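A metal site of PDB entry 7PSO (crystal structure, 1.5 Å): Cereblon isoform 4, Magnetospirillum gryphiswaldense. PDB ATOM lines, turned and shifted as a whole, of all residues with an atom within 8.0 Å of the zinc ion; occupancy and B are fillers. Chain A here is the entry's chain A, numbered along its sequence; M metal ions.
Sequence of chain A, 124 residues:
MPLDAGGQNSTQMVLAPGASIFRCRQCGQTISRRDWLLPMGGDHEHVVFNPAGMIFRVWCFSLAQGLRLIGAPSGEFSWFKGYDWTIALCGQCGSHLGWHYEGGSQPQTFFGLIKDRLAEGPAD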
ATOM      1  N   ARG A  23       2.072 -26.340   9.184  1.00  0.00           N
ATOM      2  CA  ARG A  23       2.626 -24.991   9.200  1.00  0.00           C
ATOM      3  C   ARG A  23       1.641 -23.986   8.609  1.00  0.00           C
ATOM      4  O   ARG A  23       0.797 -24.374   7.820  1.00  0.00           O
ATOM      5  CB  ARG A  23       3.930 -24.953   8.385  1.00  0.00           C
ATOM      6  CG  ARG A  23       5.036 -25.784   8.990  1.00  0.00           C
ATOM      7  CD  ARG A  23       6.365 -25.661   8.211  1.00  0.00           C
ATOM      8  NE  ARG A  23       7.386 -26.434   8.901  1.00  0.00           N
ATOM      9  CZ  ARG A  23       7.963 -26.085  10.012  1.00  0.00           C
ATOM     10  NH1 ARG A  23       7.764 -24.894  10.527  1.00  0.00           N
ATOM     11  NH2 ARG A  23       8.802 -26.906  10.609  1.00  0.00           N
ATOM     12  N   CYS A  24       1.818 -22.735   8.941  1.00  0.00           N
ATOM     13  CA  CYS A  24       1.055 -21.619   8.309  1.00  0.00           C
ATOM     14  C   CYS A  24       1.339 -21.640   6.799  1.00  0.00           C
ATOM     15  O   CYS A  24       2.524 -21.645   6.406  1.00  0.00           O
ATOM     16  CB  CYS A  24       1.407 -20.284   8.921  1.00  0.00           C
ATOM     17  SG  CYS A  24       0.582 -18.934   8.020  1.00  0.00           S
ATOM     18  N   ARG A  25       0.313 -21.682   5.973  1.00  0.00           N
ATOM     19  CA  ARG A  25       0.481 -21.745   4.494  1.00  0.00           C
ATOM     20  C   ARG A  25       1.160 -20.487   3.978  1.00  0.00           C
ATOM     21  O   ARG A  25       1.802 -20.530   2.900  1.00  0.00           O
ATOM     22  CB  ARG A  25      -0.923 -21.927   3.915  1.00  0.00           C
ATOM     23  CG  ARG A  25      -0.954 -21.971   2.408  1.00  0.00           C
ATOM     24  CD  ARG A  25      -2.330 -22.326   1.929  1.00  0.00           C
ATOM     25  NE  ARG A  25      -2.385 -22.185   0.482  1.00  0.00           N
ATOM     26  CZ  ARG A  25      -3.462 -22.394  -0.249  1.00  0.00           C
ATOM     27  NH1 ARG A  25      -4.589 -22.815   0.312  1.00  0.00           N
ATOM     28  NH2 ARG A  25      -3.400 -22.187  -1.560  1.00  0.00           N
ATOM     29  N   GLN A  26       0.933 -19.350   4.616  1.00  0.00           N
ATOM     30  CA  GLN A  26       1.462 -18.047   4.129  1.00  0.00           C
ATOM     31  C   GLN A  26       2.935 -17.884   4.484  1.00  0.00           C
ATOM     32  O   GLN A  26       3.652 -17.228   3.729  1.00  0.00           O
ATOM     33  CB  GLN A  26       0.552 -16.920   4.598  1.00  0.00           C
ATOM     34  CG  GLN A  26      -0.855 -17.080   4.079  1.00  0.00           C
ATOM     35  CD  GLN A  26      -0.913 -17.206   2.574  1.00  0.00           C
ATOM     36  OE1 GLN A  26      -0.259 -16.477   1.844  1.00  0.00           O
ATOM     37  NE2 GLN A  26      -1.667 -18.159   2.057  1.00  0.00           N
ATOM     38  N   CYS A  27       3.467 -18.452   5.560  1.00  0.00           N
ATOM     39  CA  CYS A  27       4.817 -18.064   6.030  1.00  0.00           C
ATOM     40  C   CYS A  27       5.620 -19.210   6.585  1.00  0.00           C
ATOM     41  O   CYS A  27       6.850 -19.010   6.784  1.00  0.00           O
ATOM     42  CB  CYS A  27       4.739 -16.942   7.047  1.00  0.00           C
ATOM     43  SG  CYS A  27       4.127 -17.517   8.674  1.00  0.00           S
ATOM     44  N   GLY A  28       5.028 -20.382   6.903  1.00  0.00           N
ATOM     45  CA  GLY A  28       5.834 -21.508   7.385  1.00  0.00           C
ATOM     46  C   GLY A  28       5.920 -21.648   8.881  1.00  0.00           C
ATOM     47  O   GLY A  28       6.507 -22.641   9.333  1.00  0.00           O
ATOM     48  N   GLN A  29       5.354 -20.703   9.642  1.00  0.00           N
ATOM     49  CA  GLN A  29       5.345 -20.820  11.112  1.00  0.00           C
ATOM     50  C   GLN A  29       4.862 -22.218  11.521  1.00  0.00           C
ATOM     51  O   GLN A  29       3.869 -22.670  10.998  1.00  0.00           O
ATOM     52  CB  GLN A  29       4.424 -19.748  11.710  1.00  0.00           C
ATOM     53  CG  GLN A  29       4.181 -19.914  13.212  1.00  0.00           C
ATOM     54  CD  GLN A  29       5.210 -19.177  14.039  1.00  0.00           C
ATOM     55  OE1 GLN A  29       6.388 -19.271  13.791  1.00  0.00           O
ATOM     56  NE2 GLN A  29       4.773 -18.389  14.992  1.00  0.00           N
ATOM     57  N   THR A  30       5.546 -22.914  12.429  1.00  0.00           N
ATOM     58  CA  THR A  30       5.052 -24.195  12.974  1.00  0.00           C
ATOM     59  C   THR A  30       3.762 -23.951  13.769  1.00  0.00           C
ATOM     60  O   THR A  30       3.809 -23.072  14.647  1.00  0.00           O
ATOM     61  CB  THR A  30       6.068 -24.885  13.899  1.00  0.00           C
ATOM     62  OG1 THR A  30       7.365 -24.876  13.284  1.00  0.00           O
ATOM     63  CG2 THR A  30       5.683 -26.312  14.139  1.00  0.00           C
ATOM     64  N   ILE A  31       2.692 -24.686  13.454  1.00  0.00           N
ATOM     65  CA  ILE A  31       1.384 -24.498  14.142  1.00  0.00           C
ATOM     66  C   ILE A  31       0.927 -25.753  14.891  1.00  0.00           C
ATOM     67  O   ILE A  31       0.544 -25.632  16.037  1.00  0.00           O
ATOM     68  CB  ILE A  31       0.320 -24.005  13.153  1.00  0.00           C
ATOM     69  CG1 ILE A  31       0.691 -22.715  12.441  1.00  0.00           C
ATOM     70  CG2 ILE A  31      -1.002 -23.885  13.892  1.00  0.00           C
ATOM     71  CD1 ILE A  31       0.834 -21.524  13.346  1.00  0.00           C
ATOM     72  N   GLY A  66       2.547 -21.300  18.002  1.00  0.00           N
ATOM     73  CA  GLY A  66       2.907 -20.350  16.947  1.00  0.00           C
ATOM     74  C   GLY A  66       1.801 -19.376  16.620  1.00  0.00           C
ATOM     75  O   GLY A  66       1.888 -18.671  15.589  1.00  0.00           O
ATOM     76  N   LEU A  67       0.707 -19.393  17.385  1.00  0.00           N
ATOM     77  CA  LEU A  67      -0.448 -18.509  17.133  1.00  0.00           C
ATOM     78  C   LEU A  67      -0.336 -17.319  18.072  1.00  0.00           C
ATOM     79  O   LEU A  67       0.489 -17.312  18.973  1.00  0.00           O
ATOM     80  CB  LEU A  67      -1.758 -19.241  17.402  1.00  0.00           C
ATOM     81  CG  LEU A  67      -2.004 -20.446  16.526  1.00  0.00           C
ATOM     82  CD1 LEU A  67      -3.020 -21.382  17.189  1.00  0.00           C
ATOM     83  CD2 LEU A  67      -2.352 -20.058  15.087  1.00  0.00           C
ATOM     84  N   LEU A  89      -4.580 -15.862  15.281  1.00  0.00           N
ATOM     85  CA  LEU A  89      -3.772 -15.464  14.095  1.00  0.00           C
ATOM     86  C   LEU A  89      -2.490 -16.299  14.139  1.00  0.00           C
ATOM     87  O   LEU A  89      -1.989 -16.629  15.200  1.00  0.00           O
ATOM     88  CB  LEU A  89      -3.473 -13.976  14.143  1.00  0.00           C
ATOM     89  CG  LEU A  89      -4.702 -13.049  14.214  1.00  0.00           C
ATOM     90  CD1 LEU A  89      -4.234 -11.608  14.201  1.00  0.00           C
ATOM     91  CD2 LEU A  89      -5.709 -13.336  13.120  1.00  0.00           C
ATOM     92  N   CYS A  90      -1.920 -16.537  12.959  1.00  0.00           N
ATOM     93  CA  CYS A  90      -0.481 -16.908  12.839  1.00  0.00           C
ATOM     94  C   CYS A  90       0.317 -15.848  13.611  1.00  0.00           C
ATOM     95  O   CYS A  90       0.215 -14.632  13.310  1.00  0.00           O
ATOM     96  CB  CYS A  90      -0.045 -16.924  11.385  1.00  0.00           C
ATOM     97  SG  CYS A  90       1.702 -17.375  11.293  1.00  0.00           S
ATOM     98  N   GLY A  91       1.093 -16.258  14.603  1.00  0.00           N
ATOM     99  CA  GLY A  91       1.845 -15.308  15.428  1.00  0.00           C
ATOM    100  C   GLY A  91       3.008 -14.715  14.662  1.00  0.00           C
ATOM    101  O   GLY A  91       3.517 -13.688  15.114  1.00  0.00           O
ATOM    102  N   GLN A  92       3.348 -15.288  13.502  1.00  0.00           N
ATOM    103  CA  GLN A  92       4.458 -14.761  12.660  1.00  0.00           C
ATOM    104  C   GLN A  92       3.868 -13.767  11.664  1.00  0.00           C
ATOM    105  O   GLN A  92       4.228 -12.594  11.713  1.00  0.00           O
ATOM    106  CB  GLN A  92       5.200 -15.910  11.977  1.00  0.00           C
ATOM    107  CG  GLN A  92       6.411 -15.458  11.155  1.00  0.00           C
ATOM    108  CD  GLN A  92       7.388 -16.596  10.989  1.00  0.00           C
ATOM    109  OE1 GLN A  92       8.337 -16.747  11.763  1.00  0.00           O
ATOM    110  NE2 GLN A  92       7.101 -17.500  10.074  1.00  0.00           N
ATOM    111  N   CYS A  93       2.909 -14.160  10.818  1.00  0.00           N
ATOM    112  CA  CYS A  93       2.502 -13.300   9.687  1.00  0.00           C
ATOM    113  C   CYS A  93       1.137 -12.639   9.876  1.00  0.00           C
ATOM    114  O   CYS A  93       0.779 -11.821   9.026  1.00  0.00           O
ATOM    115  CB  CYS A  93       2.540 -14.091   8.399  1.00  0.00           C
ATOM    116  SG  CYS A  93       1.119 -15.198   8.127  1.00  0.00           S
ATOM    117  N   GLY A  94       0.356 -13.049  10.868  1.00  0.00           N
ATOM    118  CA  GLY A  94      -0.948 -12.424  11.123  1.00  0.00           C
ATOM    119  C   GLY A  94      -2.090 -13.077  10.356  1.00  0.00           C
ATOM    120  O   GLY A  94      -3.234 -12.600  10.536  1.00  0.00           O
ATOM    121  N   SER A  95      -1.866 -14.077   9.519  1.00  0.00           N
ATOM    122  CA  SER A  95      -2.911 -14.830   8.784  1.00  0.00           C
ATOM    123  C   SER A  95      -3.937 -15.354   9.800  1.00  0.00           C
ATOM    124  O   SER A  95      -3.568 -15.867  10.857  1.00  0.00           O
ATOM    125  CB  SER A  95      -2.334 -15.972   8.033  1.00  0.00           C
ATOM    126  OG  SER A  95      -3.322 -16.681   7.313  1.00  0.00           O
ATOM    127  N   HIS A  96      -5.211 -15.181   9.496  1.00  0.00           N
ATOM    128  CA  HIS A  96      -6.255 -15.752  10.375  1.00  0.00           C
ATOM    129  C   HIS A  96      -6.348 -17.255  10.199  1.00  0.00           C
ATOM    130  O   HIS A  96      -6.818 -17.753   9.174  1.00  0.00           O
ATOM    131  CB  HIS A  96      -7.570 -15.066  10.109  1.00  0.00           C
ATOM    132  CG  HIS A  96      -8.629 -15.670  10.929  1.00  0.00           C
ATOM    133  ND1 HIS A  96      -9.943 -15.652  10.520  1.00  0.00           N
ATOM    134  CD2 HIS A  96      -8.586 -16.239  12.164  1.00  0.00           C
ATOM    135  CE1 HIS A  96     -10.677 -16.207  11.477  1.00  0.00           C
ATOM    136  NE2 HIS A  96      -9.877 -16.597  12.472  1.00  0.00           N
ATOM    137  N   LEU A  97      -5.815 -18.038  11.161  1.00  0.00           N
ATOM    138  CA  LEU A  97      -5.713 -19.471  11.014  1.00  0.00           C
ATOM    139  C   LEU A  97      -6.896 -20.174  11.693  1.00  0.00           C
ATOM    140  O   LEU A  97      -7.101 -21.323  11.378  1.00  0.00           O
ATOM    141  CB  LEU A  97      -4.382 -19.975  11.596  1.00  0.00           C
ATOM    142  CG  LEU A  97      -3.127 -19.507  10.873  1.00  0.00           C
ATOM    143  CD1 LEU A  97      -1.907 -20.268  11.357  1.00  0.00           C
ATOM    144  CD2 LEU A  97      -3.230 -19.622   9.389  1.00  0.00           C
ATOM    145  N   ARG A 117      -5.779 -23.239   5.293  1.00  0.00           N
ATOM    146  CA  ARG A 117      -4.814 -22.152   5.630  1.00  0.00           C
ATOM    147  C   ARG A 117      -3.551 -22.724   6.259  1.00  0.00           C
ATOM    148  O   ARG A 117      -2.675 -21.927   6.686  1.00  0.00           O
ATOM    149  CB  ARG A 117      -5.491 -21.119   6.512  1.00  0.00           C
ATOM    150  CG  ARG A 117      -6.719 -20.536   5.806  1.00  0.00           C
ATOM    151  CD  ARG A 117      -7.178 -19.272   6.462  1.00  0.00           C
ATOM    152  NE  ARG A 117      -8.481 -18.943   5.860  1.00  0.00           N
ATOM    153  CZ  ARG A 117      -9.232 -17.905   6.225  1.00  0.00           C
ATOM    154  NH1 ARG A 117      -8.844 -17.115   7.210  1.00  0.00           N
ATOM    155  NH2 ARG A 117     -10.377 -17.680   5.571  1.00  0.00           N
HETATM  156 ZN    ZN M   1       1.861 -17.251   8.944  1.00  0.00          ZN
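Along chain A the residues within 4 Å of the zinc ion span positions 24 to 93. The nearest printed residue that does not touch the zinc ion is Ser 95 (4.5 Å).
The side-chain sulfur of Cys 27 sits close to the backbone NH of Gln 29 (3.5 Å). SG of Cys 27 sits close to NE2 of Gln 92, 3.3 Å away. The backbone NH of Cys 24 is in hydrogen-bond range of the backbone carbonyl oxygen of Gln 29 (2.9 Å). N of Gln 26 lies close to SG of Cys 24 (3.4 Å). The backbone NH (N) of Ser 95 sits close to the side-chain sulfur (SG) of Cys 93. The backbone NH of Cys 90 lies within hydrogen-bond range of the backbone carbonyl oxygen of Ser 95 (2.8 Å). SG of Cys 90 lies close to N of Gln 92 (3.5 Å).
The zinc ion is bound by the side-chain sulfur of Cys 27 (2.3 Å), the side-chain sulfur of Cys 24 (2.3 Å), the side-chain sulfur of Cys 93 (2.3 Å) and the side-chain sulfur of Cys 90 (2.4 Å).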
